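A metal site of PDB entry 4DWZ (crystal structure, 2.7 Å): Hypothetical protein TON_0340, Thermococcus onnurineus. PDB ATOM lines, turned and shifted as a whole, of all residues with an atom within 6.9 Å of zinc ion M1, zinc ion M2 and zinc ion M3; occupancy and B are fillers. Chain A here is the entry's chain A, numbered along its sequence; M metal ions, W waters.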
ATOM      1  N   PHE A  50      -1.158 -24.209 -32.441  1.00  0.00           N
ATOM      2  CA  PHE A  50       0.186 -24.000 -31.896  1.00  0.00           C
ATOM      3  C   PHE A  50       0.910 -25.349 -31.825  1.00  0.00           C
ATOM      4  O   PHE A  50       0.641 -26.166 -30.956  1.00  0.00           O
ATOM      5  CB  PHE A  50       0.074 -23.381 -30.498  1.00  0.00           C
ATOM      6  CG  PHE A  50       1.300 -22.648 -30.057  1.00  0.00           C
ATOM      7  CD1 PHE A  50       1.328 -21.261 -30.063  1.00  0.00           C
ATOM      8  CD2 PHE A  50       2.435 -23.354 -29.668  1.00  0.00           C
ATOM      9  CE1 PHE A  50       2.478 -20.582 -29.684  1.00  0.00           C
ATOM     10  CE2 PHE A  50       3.592 -22.680 -29.291  1.00  0.00           C
ATOM     11  CZ  PHE A  50       3.607 -21.295 -29.300  1.00  0.00           C
ATOM     12  N   ILE A  52       3.519 -28.224 -30.940  1.00  0.00           N
ATOM     13  CA  ILE A  52       4.274 -28.469 -29.710  1.00  0.00           C
ATOM     14  C   ILE A  52       5.457 -29.402 -29.903  1.00  0.00           C
ATOM     15  O   ILE A  52       5.301 -30.566 -30.269  1.00  0.00           O
ATOM     16  CB  ILE A  52       3.340 -29.039 -28.622  1.00  0.00           C
ATOM     17  CG1 ILE A  52       2.345 -27.959 -28.217  1.00  0.00           C
ATOM     18  CG2 ILE A  52       4.138 -29.479 -27.390  1.00  0.00           C
ATOM     19  CD1 ILE A  52       1.332 -28.415 -27.263  1.00  0.00           C
ATOM     20  N   GLU A  59      -1.708 -28.089 -30.392  1.00  0.00           N
ATOM     21  CA  GLU A  59      -2.149 -28.119 -29.025  1.00  0.00           C
ATOM     22  C   GLU A  59      -3.670 -27.985 -28.878  1.00  0.00           C
ATOM     23  O   GLU A  59      -4.361 -27.572 -29.807  1.00  0.00           O
ATOM     24  CB  GLU A  59      -1.459 -26.974 -28.285  1.00  0.00           C
ATOM     25  CG  GLU A  59      -1.731 -26.929 -26.827  1.00  0.00           C
ATOM     26  CD  GLU A  59      -1.379 -25.584 -26.261  1.00  0.00           C
ATOM     27  OE1 GLU A  59      -0.383 -24.982 -26.740  1.00  0.00           O
ATOM     28  OE2 GLU A  59      -2.090 -25.137 -25.333  1.00  0.00           O
ATOM     29  N   THR A  60      -4.140 -28.288 -27.679  1.00  0.00           N
ATOM     30  CA  THR A  60      -5.546 -28.255 -27.299  1.00  0.00           C
ATOM     31  C   THR A  60      -6.067 -26.839 -26.977  1.00  0.00           C
ATOM     32  O   THR A  60      -7.274 -26.584 -27.032  1.00  0.00           O
ATOM     33  CB  THR A  60      -5.745 -29.177 -26.063  1.00  0.00           C
ATOM     34  OG1 THR A  60      -7.079 -29.673 -26.046  1.00  0.00           O
ATOM     35  CG2 THR A  60      -5.460 -28.425 -24.760  1.00  0.00           C
ATOM     36  N   ASP A  61      -5.166 -25.911 -26.639  1.00  0.00           N
ATOM     37  CA  ASP A  61      -5.574 -24.532 -26.356  1.00  0.00           C
ATOM     38  C   ASP A  61      -5.502 -23.707 -27.641  1.00  0.00           C
ATOM     39  O   ASP A  61      -4.473 -23.696 -28.325  1.00  0.00           O
ATOM     40  CB  ASP A  61      -4.648 -23.903 -25.304  1.00  0.00           C
ATOM     41  CG  ASP A  61      -5.026 -22.478 -24.974  1.00  0.00           C
ATOM     42  OD1 ASP A  61      -4.174 -21.736 -24.428  1.00  0.00           O
ATOM     43  OD2 ASP A  61      -6.184 -22.085 -25.256  1.00  0.00           O
ATOM     44  N   GLY A  62      -6.581 -23.029 -27.977  1.00  0.00           N
ATOM     45  CA  GLY A  62      -6.585 -22.251 -29.198  1.00  0.00           C
ATOM     46  C   GLY A  62      -7.801 -22.542 -30.049  1.00  0.00           C
ATOM     47  O   GLY A  62      -8.649 -21.671 -30.220  1.00  0.00           O
ATOM     48  N   GLU A 115      -3.950 -18.097 -29.865  1.00  0.00           N
ATOM     49  CA  GLU A 115      -2.882 -19.047 -29.584  1.00  0.00           C
ATOM     50  C   GLU A 115      -2.204 -19.627 -30.831  1.00  0.00           C
ATOM     51  O   GLU A 115      -2.368 -20.800 -31.158  1.00  0.00           O
ATOM     52  CB  GLU A 115      -3.444 -20.189 -28.724  1.00  0.00           C
ATOM     53  CG  GLU A 115      -2.390 -21.115 -28.166  1.00  0.00           C
ATOM     54  CD  GLU A 115      -1.569 -20.478 -27.068  1.00  0.00           C
ATOM     55  OE1 GLU A 115      -1.735 -19.265 -26.800  1.00  0.00           O
ATOM     56  OE2 GLU A 115      -0.727 -21.184 -26.479  1.00  0.00           O
ATOM     57  N   THR A 116      -1.428 -18.785 -31.508  1.00  0.00           N
ATOM     58  CA  THR A 116      -0.700 -19.157 -32.722  1.00  0.00           C
ATOM     59  C   THR A 116       0.744 -18.699 -32.539  1.00  0.00           C
ATOM     60  O   THR A 116       0.978 -17.553 -32.158  1.00  0.00           O
ATOM     61  CB  THR A 116      -1.279 -18.443 -33.955  1.00  0.00           C
ATOM     62  OG1 THR A 116      -2.689 -18.707 -34.031  1.00  0.00           O
ATOM     63  CG2 THR A 116      -0.624 -18.940 -35.225  1.00  0.00           C
ATOM     64  N   MET A 128       7.131 -22.657 -25.090  1.00  0.00           N
ATOM     65  CA  MET A 128       7.341 -22.055 -23.788  1.00  0.00           C
ATOM     66  C   MET A 128       8.601 -22.608 -23.109  1.00  0.00           C
ATOM     67  O   MET A 128       9.222 -21.926 -22.294  1.00  0.00           O
ATOM     68  CB  MET A 128       6.105 -22.268 -22.897  1.00  0.00           C
ATOM     69  CG  MET A 128       4.931 -21.333 -23.219  1.00  0.00           C
ATOM     70  SD  MET A 128       5.350 -19.544 -23.281  1.00  0.00           S
ATOM     71  CE  MET A 128       5.636 -19.145 -21.518  1.00  0.00           C
ATOM     72  N   VAL A 155      -4.680 -13.026 -29.289  1.00  0.00           N
ATOM     73  CA  VAL A 155      -4.957 -13.486 -27.928  1.00  0.00           C
ATOM     74  C   VAL A 155      -3.864 -14.444 -27.528  1.00  0.00           C
ATOM     75  O   VAL A 155      -3.604 -15.403 -28.253  1.00  0.00           O
ATOM     76  CB  VAL A 155      -6.289 -14.219 -27.810  1.00  0.00           C
ATOM     77  CG1 VAL A 155      -6.515 -14.631 -26.373  1.00  0.00           C
ATOM     78  CG2 VAL A 155      -7.437 -13.351 -28.290  1.00  0.00           C
ATOM     79  N   GLY A 156      -3.242 -14.216 -26.379  1.00  0.00           N
ATOM     80  CA  GLY A 156      -2.177 -15.097 -25.947  1.00  0.00           C
ATOM     81  C   GLY A 156      -2.058 -15.165 -24.443  1.00  0.00           C
ATOM     82  O   GLY A 156      -2.632 -14.341 -23.729  1.00  0.00           O
ATOM     83  N   ASP A 157      -1.298 -16.142 -23.947  1.00  0.00           N
ATOM     84  CA  ASP A 157      -1.114 -16.340 -22.526  1.00  0.00           C
ATOM     85  C   ASP A 157       0.310 -16.707 -22.083  1.00  0.00           C
ATOM     86  O   ASP A 157       0.509 -17.107 -20.946  1.00  0.00           O
ATOM     87  CB  ASP A 157      -2.086 -17.409 -22.029  1.00  0.00           C
ATOM     88  CG  ASP A 157      -1.942 -18.718 -22.772  1.00  0.00           C
ATOM     89  OD1 ASP A 157      -0.980 -18.880 -23.555  1.00  0.00           O
ATOM     90  OD2 ASP A 157      -2.794 -19.608 -22.572  1.00  0.00           O
ATOM     91  N   GLY A 158       1.295 -16.578 -22.964  1.00  0.00           N
ATOM     92  CA  GLY A 158       2.659 -16.918 -22.587  1.00  0.00           C
ATOM     93  C   GLY A 158       3.782 -16.008 -23.086  1.00  0.00           C
ATOM     94  O   GLY A 158       4.916 -16.144 -22.655  1.00  0.00           O
ATOM     95  N   GLY A 159       3.469 -15.103 -24.015  1.00  0.00           N
ATOM     96  CA  GLY A 159       4.491 -14.194 -24.521  1.00  0.00           C
ATOM     97  C   GLY A 159       5.176 -14.575 -25.832  1.00  0.00           C
ATOM     98  O   GLY A 159       5.938 -13.788 -26.367  1.00  0.00           O
ATOM     99  N   ASN A 160       4.906 -15.756 -26.363  1.00  0.00           N
ATOM    100  CA  ASN A 160       5.545 -16.194 -27.610  1.00  0.00           C
ATOM    101  C   ASN A 160       4.518 -16.403 -28.711  1.00  0.00           C
ATOM    102  O   ASN A 160       4.770 -17.117 -29.677  1.00  0.00           O
ATOM    103  CB  ASN A 160       6.279 -17.504 -27.405  1.00  0.00           C
ATOM    104  CG  ASN A 160       5.336 -18.675 -27.161  1.00  0.00           C
ATOM    105  OD1 ASN A 160       4.158 -18.481 -26.841  1.00  0.00           O
ATOM    106  ND2 ASN A 160       5.857 -19.887 -27.292  1.00  0.00           N
ATOM    107  N   GLU A 161       3.365 -15.760 -28.555  1.00  0.00           N
ATOM    108  CA  GLU A 161       2.287 -15.894 -29.521  1.00  0.00           C
ATOM    109  C   GLU A 161       2.189 -14.660 -30.418  1.00  0.00           C
ATOM    110  O   GLU A 161       2.865 -13.655 -30.203  1.00  0.00           O
ATOM    111  CB  GLU A 161       0.953 -16.117 -28.800  1.00  0.00           C
ATOM    112  CG  GLU A 161       0.949 -17.294 -27.826  1.00  0.00           C
ATOM    113  CD  GLU A 161       1.327 -16.888 -26.403  1.00  0.00           C
ATOM    114  OE1 GLU A 161       2.188 -15.997 -26.228  1.00  0.00           O
ATOM    115  OE2 GLU A 161       0.774 -17.462 -25.453  1.00  0.00           O
ATOM    116  N   ALA A 194      -4.779 -16.219 -18.760  1.00  0.00           N
ATOM    117  CA  ALA A 194      -4.103 -17.324 -18.109  1.00  0.00           C
ATOM    118  C   ALA A 194      -4.099 -18.491 -19.110  1.00  0.00           C
ATOM    119  O   ALA A 194      -3.132 -19.238 -19.186  1.00  0.00           O
ATOM    120  CB  ALA A 194      -4.844 -17.686 -16.853  1.00  0.00           C
ATOM    121  N   VAL A 195      -5.201 -18.617 -19.847  1.00  0.00           N
ATOM    122  CA  VAL A 195      -5.375 -19.651 -20.879  1.00  0.00           C
ATOM    123  C   VAL A 195      -5.998 -18.896 -22.058  1.00  0.00           C
ATOM    124  O   VAL A 195      -6.997 -18.192 -21.894  1.00  0.00           O
ATOM    125  CB  VAL A 195      -6.366 -20.805 -20.429  1.00  0.00           C
ATOM    126  CG1 VAL A 195      -6.417 -21.876 -21.510  1.00  0.00           C
ATOM    127  CG2 VAL A 195      -5.927 -21.441 -19.123  1.00  0.00           C
ATOM    128  N   SER A 196      -5.437 -19.045 -23.254  1.00  0.00           N
ATOM    129  CA  SER A 196      -5.950 -18.305 -24.398  1.00  0.00           C
ATOM    130  C   SER A 196      -7.410 -18.527 -24.781  1.00  0.00           C
ATOM    131  O   SER A 196      -8.060 -17.587 -25.233  1.00  0.00           O
ATOM    132  CB  SER A 196      -5.057 -18.517 -25.623  1.00  0.00           C
ATOM    133  OG  SER A 196      -3.763 -17.995 -25.378  1.00  0.00           O
ATOM    134  N   ASN A 197      -7.937 -19.735 -24.593  1.00  0.00           N
ATOM    135  CA  ASN A 197      -9.344 -19.956 -24.918  1.00  0.00           C
ATOM    136  C   ASN A 197     -10.229 -19.025 -24.060  1.00  0.00           C
ATOM    137  O   ASN A 197     -11.237 -18.485 -24.532  1.00  0.00           O
ATOM    138  CB  ASN A 197      -9.747 -21.419 -24.680  1.00  0.00           C
ATOM    139  CG  ASN A 197      -9.045 -22.390 -25.621  1.00  0.00           C
ATOM    140  OD1 ASN A 197      -8.964 -22.164 -26.843  1.00  0.00           O
ATOM    141  ND2 ASN A 197      -8.545 -23.483 -25.066  1.00  0.00           N
ATOM    142  N   ASP A 235      -2.464 -32.061 -25.218  1.00  0.00           N
ATOM    143  CA  ASP A 235      -2.460 -31.102 -24.121  1.00  0.00           C
ATOM    144  C   ASP A 235      -1.031 -30.574 -24.088  1.00  0.00           C
ATOM    145  O   ASP A 235      -0.086 -31.353 -23.924  1.00  0.00           O
ATOM    146  CB  ASP A 235      -2.810 -31.772 -22.787  1.00  0.00           C
ATOM    147  CG  ASP A 235      -2.792 -30.796 -21.628  1.00  0.00           C
ATOM    148  OD1 ASP A 235      -3.881 -30.358 -21.208  1.00  0.00           O
ATOM    149  OD2 ASP A 235      -1.686 -30.466 -21.132  1.00  0.00           O
ATOM    150  N   GLY A 236      -0.888 -29.272 -24.248  1.00  0.00           N
ATOM    151  CA  GLY A 236       0.416 -28.633 -24.275  1.00  0.00           C
ATOM    152  C   GLY A 236       1.401 -28.948 -23.169  1.00  0.00           C
ATOM    153  O   GLY A 236       2.602 -28.991 -23.412  1.00  0.00           O
ATOM    154  N   VAL A 237       0.913 -29.158 -21.950  1.00  0.00           N
ATOM    155  CA  VAL A 237       1.806 -29.426 -20.843  1.00  0.00           C
ATOM    156  C   VAL A 237       2.174 -30.889 -20.669  1.00  0.00           C
ATOM    157  O   VAL A 237       3.354 -31.225 -20.599  1.00  0.00           O
ATOM    158  CB  VAL A 237       1.218 -28.906 -19.521  1.00  0.00           C
ATOM    159  CG1 VAL A 237       2.248 -29.021 -18.423  1.00  0.00           C
ATOM    160  CG2 VAL A 237       0.803 -27.445 -19.680  1.00  0.00           C
ATOM    161  N   VAL A 245      -6.669 -28.811 -20.971  1.00  0.00           N
ATOM    162  CA  VAL A 245      -6.048 -27.670 -21.641  1.00  0.00           C
ATOM    163  C   VAL A 245      -4.979 -27.039 -20.766  1.00  0.00           C
ATOM    164  O   VAL A 245      -5.232 -26.729 -19.603  1.00  0.00           O
ATOM    165  CB  VAL A 245      -7.088 -26.596 -21.993  1.00  0.00           C
ATOM    166  CG1 VAL A 245      -6.433 -25.511 -22.825  1.00  0.00           C
ATOM    167  CG2 VAL A 245      -8.246 -27.207 -22.739  1.00  0.00           C
ATOM    168  N   ASP A 246      -3.801 -26.827 -21.342  1.00  0.00           N
ATOM    169  CA  ASP A 246      -2.662 -26.248 -20.632  1.00  0.00           C
ATOM    170  C   ASP A 246      -2.500 -26.885 -19.257  1.00  0.00           C
ATOM    171  O   ASP A 246      -2.353 -26.173 -18.256  1.00  0.00           O
ATOM    172  CB  ASP A 246      -2.828 -24.748 -20.493  1.00  0.00           C
ATOM    173  CG  ASP A 246      -2.732 -24.023 -21.813  1.00  0.00           C
ATOM    174  OD1 ASP A 246      -2.127 -24.570 -22.752  1.00  0.00           O
ATOM    175  OD2 ASP A 246      -3.244 -22.895 -21.915  1.00  0.00           O
ATOM    176  N   GLY A 247      -2.559 -28.214 -19.231  1.00  0.00           N
ATOM    177  CA  GLY A 247      -2.417 -28.959 -17.989  1.00  0.00           C
ATOM    178  C   GLY A 247      -3.511 -28.794 -16.951  1.00  0.00           C
ATOM    179  O   GLY A 247      -3.384 -29.310 -15.841  1.00  0.00           O
HETATM  180 ZN    ZN M   1       0.494 -19.670 -25.190  1.00  0.00          ZN
HETATM  181 ZN    ZN M   2      -2.183 -21.800 -23.508  1.00  0.00          ZN
HETATM  182 ZN    ZN M   3      -0.495 -24.715 -24.148  1.00  0.00          ZN
HETATM  183  O   HOH W   1      -0.875 -22.976 -24.868  1.00  0.00           O
HETATM  184  O   HOH W   2       1.548 -25.471 -23.134  1.00  0.00           O
HETATM  185  O   HOH W   3       2.706 -20.351 -26.021  1.00  0.00           O
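OE2 of Glu 59 sits close to N of Asp 61 (3.4 Å). The backbone NH of Glu 59 is in hydrogen-bond range of the backbone carbonyl oxygen of Phe 50 (3.1 Å). OD2 of Asp 61 lies within hydrogen-bond range of ND2 of Asn 197 (2.8 Å). The side-chain carboxylate of Glu 161 is in hydrogen-bond range of the backbone NH of Gly 158 (3.4 Å). OD1 of Asn 160 sits close to OE1 of Glu 161 (3.2 Å). OE1 of Glu 161 is in hydrogen-bond range of N of Gly 159, 2.7 Å away. The backbone NH (N) of Glu 115 sits at hydrogen-bond distance from the backbone carbonyl oxygen (O) of Val 155 (3.2 Å). N of Asp 157 lies close to OG of Ser 196 (3.4 Å).
Residues that only touch zinc ion M1: Gly 158. Four residues have an atom within 4 Å of zinc ion M1: Glu 115, Asp 157, Gly 158 and Glu 161. The nearest printed residue that does not touch zinc ion M1 is Asn 160 (4.2 Å).
Within 4 Å of zinc ion M2: Glu 59, Asp 61, Glu 115, Asp 157 and Asp 246.
Of the 26 residues printed, 2 come within 4 Å of zinc ion M3.
Zinc ion M1 is bound by OE2 of Glu 161 (2.2 Å), OE2 of Glu 115 (2.3 Å), OD1 of Asp 157 (2.3 Å) and water W3 (2.5 Å). Zinc ion M1 has four donor atoms within binding distance. Slightly farther from zinc ion M1 lies the side-chain carboxylate (OE1) of Glu 115 (2.8 Å).
Zinc ion M2 is bound by OD1 of Asp 61, OD2 of Asp 246, water W1 and OD2 of Asp 157.
Zinc ion M3 is bound by water W1 (1.9 Å), OE2 of Glu 59 (2.0 Å), OD1 of Asp 246 (2.2 Å) and water W2 (2.4 Å). Zinc ion M3 has four donor atoms within binding distance. Slightly farther from zinc ion M3 lies the side-chain carboxylate (OE1) of Glu 59 (2.6 Å).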
